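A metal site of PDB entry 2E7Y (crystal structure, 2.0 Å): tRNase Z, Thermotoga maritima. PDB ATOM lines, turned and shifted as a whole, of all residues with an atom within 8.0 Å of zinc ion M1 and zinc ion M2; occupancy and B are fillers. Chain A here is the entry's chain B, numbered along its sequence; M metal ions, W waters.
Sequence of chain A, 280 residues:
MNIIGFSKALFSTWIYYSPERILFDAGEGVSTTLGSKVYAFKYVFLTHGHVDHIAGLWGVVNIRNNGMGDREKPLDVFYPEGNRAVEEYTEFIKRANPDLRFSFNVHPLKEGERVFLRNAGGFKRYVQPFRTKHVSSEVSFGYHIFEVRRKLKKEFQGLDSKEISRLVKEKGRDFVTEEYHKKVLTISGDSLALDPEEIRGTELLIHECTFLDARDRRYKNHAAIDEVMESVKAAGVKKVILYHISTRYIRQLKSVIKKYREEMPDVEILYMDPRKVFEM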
ATOM      1  N   SER A   7       2.393  15.783 -10.475  1.00  0.00           N
ATOM      2  CA  SER A   7       1.690  14.540 -10.637  1.00  0.00           C
ATOM      3  C   SER A   7       0.925  14.524 -11.947  1.00  0.00           C
ATOM      4  O   SER A   7       0.213  15.472 -12.292  1.00  0.00           O
ATOM      5  CB  SER A   7       0.718  14.292  -9.469  1.00  0.00           C
ATOM      6  OG  SER A   7       0.084  13.016  -9.615  1.00  0.00           O
ATOM      7  N   LYS A   8       1.096  13.441 -12.682  1.00  0.00           N
ATOM      8  CA  LYS A   8       0.383  13.237 -13.933  1.00  0.00           C
ATOM      9  C   LYS A   8       0.159  11.743 -13.929  1.00  0.00           C
ATOM     10  O   LYS A   8       1.122  10.958 -13.962  1.00  0.00           O
ATOM     11  CB  LYS A   8       1.243  13.653 -15.130  1.00  0.00           C
ATOM     12  CG  LYS A   8       0.590  13.434 -16.502  1.00  0.00           C
ATOM     13  CD  LYS A   8       1.669  13.592 -17.566  1.00  0.00           C
ATOM     14  CE  LYS A   8       1.127  13.824 -18.945  1.00  0.00           C
ATOM     15  NZ  LYS A   8       2.282  14.218 -19.794  1.00  0.00           N
ATOM     16  N   ALA A   9      -1.098  11.356 -13.847  1.00  0.00           N
ATOM     17  CA  ALA A   9      -1.470   9.939 -13.796  1.00  0.00           C
ATOM     18  C   ALA A   9      -0.663   9.066 -14.739  1.00  0.00           C
ATOM     19  O   ALA A   9      -0.581   9.356 -15.913  1.00  0.00           O
ATOM     20  CB  ALA A   9      -2.979   9.764 -14.109  1.00  0.00           C
ATOM     21  N   LEU A  10      -0.128   7.977 -14.198  1.00  0.00           N
ATOM     22  CA  LEU A  10       0.635   6.994 -14.971  1.00  0.00           C
ATOM     23  C   LEU A  10       2.056   7.406 -15.422  1.00  0.00           C
ATOM     24  O   LEU A  10       2.842   6.547 -15.815  1.00  0.00           O
ATOM     25  CB  LEU A  10      -0.172   6.556 -16.211  1.00  0.00           C
ATOM     26  CG  LEU A  10      -1.669   6.212 -16.110  1.00  0.00           C
ATOM     27  CD1 LEU A  10      -2.215   6.034 -17.503  1.00  0.00           C
ATOM     28  CD2 LEU A  10      -1.916   4.954 -15.294  1.00  0.00           C
ATOM     29  N   PHE A  11       2.375   8.700 -15.360  1.00  0.00           N
ATOM     30  CA  PHE A  11       3.701   9.178 -15.783  1.00  0.00           C
ATOM     31  C   PHE A  11       4.662   9.489 -14.627  1.00  0.00           C
ATOM     32  O   PHE A  11       5.779   8.982 -14.566  1.00  0.00           O
ATOM     33  CB  PHE A  11       3.550  10.421 -16.669  1.00  0.00           C
ATOM     34  CG  PHE A  11       2.971  10.126 -18.039  1.00  0.00           C
ATOM     35  CD1 PHE A  11       1.607   9.902 -18.203  1.00  0.00           C
ATOM     36  CD2 PHE A  11       3.804  10.052 -19.161  1.00  0.00           C
ATOM     37  CE1 PHE A  11       1.082   9.618 -19.485  1.00  0.00           C
ATOM     38  CE2 PHE A  11       3.283   9.770 -20.427  1.00  0.00           C
ATOM     39  CZ  PHE A  11       1.924   9.555 -20.581  1.00  0.00           C
ATOM     40  N   SER A  12       4.235  10.331 -13.705  1.00  0.00           N
ATOM     41  CA  SER A  12       5.096  10.665 -12.592  1.00  0.00           C
ATOM     42  C   SER A  12       4.322  11.373 -11.499  1.00  0.00           C
ATOM     43  O   SER A  12       3.488  12.222 -11.771  1.00  0.00           O
ATOM     44  CB  SER A  12       6.224  11.579 -13.067  1.00  0.00           C
ATOM     45  OG  SER A  12       7.057  12.014 -11.984  1.00  0.00           O
ATOM     46  N   THR A  13       4.642  11.019 -10.264  1.00  0.00           N
ATOM     47  CA  THR A  13       4.044  11.601  -9.080  1.00  0.00           C
ATOM     48  C   THR A  13       5.077  11.664  -7.965  1.00  0.00           C
ATOM     49  O   THR A  13       5.722  10.663  -7.637  1.00  0.00           O
ATOM     50  CB  THR A  13       2.853  10.755  -8.543  1.00  0.00           C
ATOM     51  OG1 THR A  13       1.743  10.870  -9.433  1.00  0.00           O
ATOM     52  CG2 THR A  13       2.422  11.239  -7.143  1.00  0.00           C
ATOM     53  N   ASP A  25       6.571   9.583  -2.346  1.00  0.00           N
ATOM     54  CA  ASP A  25       6.675   9.057  -3.693  1.00  0.00           C
ATOM     55  C   ASP A  25       7.833   9.709  -4.413  1.00  0.00           C
ATOM     56  O   ASP A  25       8.315  10.772  -4.027  1.00  0.00           O
ATOM     57  CB  ASP A  25       5.364   9.233  -4.443  1.00  0.00           C
ATOM     58  CG  ASP A  25       4.400   8.115  -4.140  1.00  0.00           C
ATOM     59  OD1 ASP A  25       3.236   8.203  -4.538  1.00  0.00           O
ATOM     60  OD2 ASP A  25       4.832   7.123  -3.514  1.00  0.00           O
ATOM     61  N   THR A  47       4.180   5.232  -1.500  1.00  0.00           N
ATOM     62  CA  THR A  47       2.818   4.718  -1.400  1.00  0.00           C
ATOM     63  C   THR A  47       2.726   3.375  -2.096  1.00  0.00           C
ATOM     64  O   THR A  47       1.869   2.562  -1.775  1.00  0.00           O
ATOM     65  CB  THR A  47       1.804   5.693  -1.990  1.00  0.00           C
ATOM     66  OG1 THR A  47       2.008   5.859  -3.402  1.00  0.00           O
ATOM     67  CG2 THR A  47       1.950   7.035  -1.290  1.00  0.00           C
ATOM     68  N   HIS A  48       3.635   3.133  -3.036  1.00  0.00           N
ATOM     69  CA  HIS A  48       3.706   1.865  -3.753  1.00  0.00           C
ATOM     70  C   HIS A  48       4.868   1.842  -4.762  1.00  0.00           C
ATOM     71  O   HIS A  48       5.669   2.775  -4.813  1.00  0.00           O
ATOM     72  CB  HIS A  48       2.377   1.472  -4.421  1.00  0.00           C
ATOM     73  CG  HIS A  48       1.858   2.448  -5.426  1.00  0.00           C
ATOM     74  ND1 HIS A  48       1.869   3.814  -5.210  1.00  0.00           N
ATOM     75  CD2 HIS A  48       1.243   2.257  -6.625  1.00  0.00           C
ATOM     76  CE1 HIS A  48       1.267   4.419  -6.225  1.00  0.00           C
ATOM     77  NE2 HIS A  48       0.884   3.496  -7.098  1.00  0.00           N
ATOM     78  N   GLY A  49       4.949   0.750  -5.515  1.00  0.00           N
ATOM     79  CA  GLY A  49       6.044   0.526  -6.433  1.00  0.00           C
ATOM     80  C   GLY A  49       5.870   0.593  -7.940  1.00  0.00           C
ATOM     81  O   GLY A  49       6.708   0.077  -8.665  1.00  0.00           O
ATOM     82  N   HIS A  50       4.789   1.208  -8.413  1.00  0.00           N
ATOM     83  CA  HIS A  50       4.588   1.353  -9.845  1.00  0.00           C
ATOM     84  C   HIS A  50       5.616   2.366 -10.331  1.00  0.00           C
ATOM     85  O   HIS A  50       5.957   3.326  -9.638  1.00  0.00           O
ATOM     86  CB  HIS A  50       3.176   1.860 -10.148  1.00  0.00           C
ATOM     87  CG  HIS A  50       2.135   0.779 -10.113  1.00  0.00           C
ATOM     88  ND1 HIS A  50       0.794   1.038 -10.217  1.00  0.00           N
ATOM     89  CD2 HIS A  50       2.256  -0.570  -9.986  1.00  0.00           C
ATOM     90  CE1 HIS A  50       0.116  -0.096 -10.142  1.00  0.00           C
ATOM     91  NE2 HIS A  50       0.983  -1.084 -10.005  1.00  0.00           N
ATOM     92  N   VAL A  51       6.083   2.172 -11.566  1.00  0.00           N
ATOM     93  CA  VAL A  51       7.110   3.026 -12.140  1.00  0.00           C
ATOM     94  C   VAL A  51       6.913   4.521 -11.959  1.00  0.00           C
ATOM     95  O   VAL A  51       7.865   5.218 -11.594  1.00  0.00           O
ATOM     96  CB  VAL A  51       7.315   2.704 -13.670  1.00  0.00           C
ATOM     97  CG1 VAL A  51       6.032   2.944 -14.424  1.00  0.00           C
ATOM     98  CG2 VAL A  51       8.445   3.553 -14.252  1.00  0.00           C
ATOM     99  N   ASP A  52       5.691   5.014 -12.172  1.00  0.00           N
ATOM    100  CA  ASP A  52       5.419   6.460 -12.020  1.00  0.00           C
ATOM    101  C   ASP A  52       5.498   7.042 -10.612  1.00  0.00           C
ATOM    102  O   ASP A  52       5.386   8.252 -10.424  1.00  0.00           O
ATOM    103  CB  ASP A  52       4.083   6.854 -12.683  1.00  0.00           C
ATOM    104  CG  ASP A  52       2.864   6.119 -12.123  1.00  0.00           C
ATOM    105  OD1 ASP A  52       2.924   4.884 -11.917  1.00  0.00           O
ATOM    106  OD2 ASP A  52       1.817   6.791 -11.928  1.00  0.00           O
ATOM    107  N   HIS A  53       5.712   6.178  -9.640  1.00  0.00           N
ATOM    108  CA  HIS A  53       5.852   6.605  -8.253  1.00  0.00           C
ATOM    109  C   HIS A  53       7.244   6.337  -7.686  1.00  0.00           C
ATOM    110  O   HIS A  53       7.531   6.734  -6.555  1.00  0.00           O
ATOM    111  CB  HIS A  53       4.802   5.895  -7.397  1.00  0.00           C
ATOM    112  CG  HIS A  53       3.428   6.369  -7.658  1.00  0.00           C
ATOM    113  ND1 HIS A  53       2.824   7.368  -6.909  1.00  0.00           N
ATOM    114  CD2 HIS A  53       2.542   6.053  -8.629  1.00  0.00           C
ATOM    115  CE1 HIS A  53       1.640   7.635  -7.415  1.00  0.00           C
ATOM    116  NE2 HIS A  53       1.438   6.848  -8.459  1.00  0.00           N
ATOM    117  N   SER A 140      -0.547  -1.306  -1.512  1.00  0.00           N
ATOM    118  CA  SER A 140      -0.539   0.151  -1.589  1.00  0.00           C
ATOM    119  C   SER A 140      -0.915   0.814  -0.232  1.00  0.00           C
ATOM    120  O   SER A 140      -1.849   0.376   0.439  1.00  0.00           O
ATOM    121  CB  SER A 140      -1.521   0.576  -2.695  1.00  0.00           C
ATOM    122  OG  SER A 140      -1.520   1.973  -2.889  1.00  0.00           O
ATOM    123  N   GLY A 189      -2.362   8.401  -1.910  1.00  0.00           N
ATOM    124  CA  GLY A 189      -1.594   7.469  -2.703  1.00  0.00           C
ATOM    125  C   GLY A 189      -2.603   7.094  -3.772  1.00  0.00           C
ATOM    126  O   GLY A 189      -3.614   7.784  -3.895  1.00  0.00           O
ATOM    127  N   ASP A 190      -2.374   6.051  -4.546  1.00  0.00           N
ATOM    128  CA  ASP A 190      -3.366   5.684  -5.549  1.00  0.00           C
ATOM    129  C   ASP A 190      -4.448   4.836  -4.890  1.00  0.00           C
ATOM    130  O   ASP A 190      -4.125   3.904  -4.159  1.00  0.00           O
ATOM    131  CB  ASP A 190      -2.733   4.879  -6.696  1.00  0.00           C
ATOM    132  CG  ASP A 190      -1.846   5.737  -7.577  1.00  0.00           C
ATOM    133  OD1 ASP A 190      -1.356   5.211  -8.602  1.00  0.00           O
ATOM    134  OD2 ASP A 190      -1.627   6.921  -7.253  1.00  0.00           O
ATOM    135  N   SER A 191      -5.714   5.164  -5.131  1.00  0.00           N
ATOM    136  CA  SER A 191      -6.840   4.416  -4.575  1.00  0.00           C
ATOM    137  C   SER A 191      -8.202   5.029  -4.880  1.00  0.00           C
ATOM    138  O   SER A 191      -8.296   6.123  -5.456  1.00  0.00           O
ATOM    139  CB  SER A 191      -6.717   4.271  -3.051  1.00  0.00           C
ATOM    140  OG  SER A 191      -7.079   5.464  -2.383  1.00  0.00           O
ATOM    141  N   GLU A 208      -5.920  11.392  -4.739  1.00  0.00           N
ATOM    142  CA  GLU A 208      -5.814  11.169  -6.166  1.00  0.00           C
ATOM    143  C   GLU A 208      -7.138  11.419  -6.844  1.00  0.00           C
ATOM    144  O   GLU A 208      -8.198  11.177  -6.273  1.00  0.00           O
ATOM    145  CB  GLU A 208      -5.343   9.750  -6.456  1.00  0.00           C
ATOM    146  CG  GLU A 208      -6.356   8.690  -6.184  1.00  0.00           C
ATOM    147  CD  GLU A 208      -6.554   7.808  -7.380  1.00  0.00           C
ATOM    148  OE1 GLU A 208      -7.218   8.254  -8.347  1.00  0.00           O
ATOM    149  OE2 GLU A 208      -6.032   6.676  -7.364  1.00  0.00           O
ATOM    150  N   THR A 210      -7.761  10.572 -10.564  1.00  0.00           N
ATOM    151  CA  THR A 210      -7.467  10.072 -11.909  1.00  0.00           C
ATOM    152  C   THR A 210      -8.538  10.346 -12.961  1.00  0.00           C
ATOM    153  O   THR A 210      -8.207  10.679 -14.096  1.00  0.00           O
ATOM    154  CB  THR A 210      -7.159   8.567 -11.877  1.00  0.00           C
ATOM    155  OG1 THR A 210      -6.186   8.295 -10.860  1.00  0.00           O
ATOM    156  CG2 THR A 210      -6.611   8.116 -13.203  1.00  0.00           C
ATOM    157  N   ASN A 221      -9.760   1.209  -9.603  1.00  0.00           N
ATOM    158  CA  ASN A 221      -8.467   1.251  -8.936  1.00  0.00           C
ATOM    159  C   ASN A 221      -8.116   2.716  -8.730  1.00  0.00           C
ATOM    160  O   ASN A 221      -7.086   3.045  -8.127  1.00  0.00           O
ATOM    161  CB  ASN A 221      -7.395   0.587  -9.799  1.00  0.00           C
ATOM    162  CG  ASN A 221      -7.955   0.032 -11.086  1.00  0.00           C
ATOM    163  OD1 ASN A 221      -8.738  -0.913 -11.074  1.00  0.00           O
ATOM    164  ND2 ASN A 221      -7.551   0.610 -12.211  1.00  0.00           N
ATOM    165  N   HIS A 222      -8.978   3.587  -9.237  1.00  0.00           N
ATOM    166  CA  HIS A 222      -8.784   5.022  -9.119  1.00  0.00           C
ATOM    167  C   HIS A 222     -10.099   5.734  -8.855  1.00  0.00           C
ATOM    168  O   HIS A 222     -11.158   5.264  -9.246  1.00  0.00           O
ATOM    169  CB  HIS A 222      -8.133   5.565 -10.380  1.00  0.00           C
ATOM    170  CG  HIS A 222      -6.714   5.117 -10.554  1.00  0.00           C
ATOM    171  ND1 HIS A 222      -5.685   5.611  -9.774  1.00  0.00           N
ATOM    172  CD2 HIS A 222      -6.163   4.175 -11.351  1.00  0.00           C
ATOM    173  CE1 HIS A 222      -4.560   4.980 -10.090  1.00  0.00           C
ATOM    174  NE2 HIS A 222      -4.829   4.110 -11.041  1.00  0.00           N
ATOM    175  N   TYR A 243      -4.789  15.370  -7.016  1.00  0.00           N
ATOM    176  CA  TYR A 243      -3.635  15.064  -7.855  1.00  0.00           C
ATOM    177  C   TYR A 243      -3.808  13.763  -8.601  1.00  0.00           C
ATOM    178  O   TYR A 243      -4.879  13.155  -8.594  1.00  0.00           O
ATOM    179  CB  TYR A 243      -2.338  15.036  -7.030  1.00  0.00           C
ATOM    180  CG  TYR A 243      -2.117  13.809  -6.164  1.00  0.00           C
ATOM    181  CD1 TYR A 243      -0.939  13.065  -6.275  1.00  0.00           C
ATOM    182  CD2 TYR A 243      -3.045  13.428  -5.194  1.00  0.00           C
ATOM    183  CE1 TYR A 243      -0.675  11.978  -5.449  1.00  0.00           C
ATOM    184  CE2 TYR A 243      -2.793  12.317  -4.351  1.00  0.00           C
ATOM    185  CZ  TYR A 243      -1.602  11.604  -4.487  1.00  0.00           C
ATOM    186  OH  TYR A 243      -1.320  10.519  -3.684  1.00  0.00           O
ATOM    187  N   HIS A 244      -2.731  13.332  -9.260  1.00  0.00           N
ATOM    188  CA  HIS A 244      -2.740  12.114 -10.035  1.00  0.00           C
ATOM    189  C   HIS A 244      -3.806  12.212 -11.120  1.00  0.00           C
ATOM    190  O   HIS A 244      -4.458  11.224 -11.490  1.00  0.00           O
ATOM    191  CB  HIS A 244      -3.003  10.922  -9.140  1.00  0.00           C
ATOM    192  CG  HIS A 244      -2.559   9.636  -9.752  1.00  0.00           C
ATOM    193  ND1 HIS A 244      -3.393   8.835 -10.507  1.00  0.00           N
ATOM    194  CD2 HIS A 244      -1.361   9.008  -9.733  1.00  0.00           C
ATOM    195  CE1 HIS A 244      -2.729   7.776 -10.927  1.00  0.00           C
ATOM    196  NE2 HIS A 244      -1.491   7.857 -10.467  1.00  0.00           N
HETATM  197 ZN    ZN M   1      -0.198   3.034  -9.152  1.00  0.00          ZN
HETATM  198 ZN    ZN M   2      -0.137   6.246  -9.854  1.00  0.00          ZN
HETATM  199  O   HOH W   1       0.013   4.889 -11.373  1.00  0.00           O
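Zinc ion M2 is bound by OD1 of Asp 190 (2.0 Å). Water W1 binds zinc ion M2 (2.0 Å). A ring nitrogen (NE2) of His 53 binds zinc ion M2, at 2.2 Å. NE2 of His 244 is bound to zinc ion M2, at 2.2 Å. Zinc ion M2 has four donor atoms within binding distance.
Zinc ion M1 is bound by NE2 of His 48 (2.4 Å), ND1 of His 50 (2.5 Å) and OD1 of Asp 190 (2.5 Å).
OD2 of Asp 52 touches zinc ion M2 (2.9 Å). Of the 25 residues printed, 4 come within 4 Å of zinc ion M2. The nearest printed residue that does not touch zinc ion M2 is His 48 (4.02 Å).
A ring nitrogen (NE2) of His 53 sits close to the side-chain carboxylate (OD2) of Asp 52, 3.5 Å away. The backbone NH (N) of Leu 10 sits at hydrogen-bond distance from the side-chain carboxylate (OD2) of Asp 52 (3.2 Å). A ring nitrogen (ND1) of His 53 sits at hydrogen-bond distance from the side-chain carboxylate (OD1) of Asp 25. The side-chain hydroxyl (OG) of Ser 7 sits at hydrogen-bond distance from the backbone NH (N) of His 244, 2.9 Å away. O of Asp 190 lies within hydrogen-bond range of OG of Ser 140 (3.5 Å). The backbone carbonyl oxygen (O) of Asp 52 lies within hydrogen-bond range of the backbone NH (N) of Thr 13 (2.9 Å). A ring nitrogen (ND1) of His 48 is in hydrogen-bond range of the side-chain hydroxyl (OG1) of Thr 47 (2.7 Å). ND1 of His 244 lies within hydrogen-bond range of OG1 of Thr 210.
Within 4 Å of zinc ion M1: His 48, His 50 and Asp 190. Along chain A the residues within 4 Å of zinc ion M1 span positions 48 to 190.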
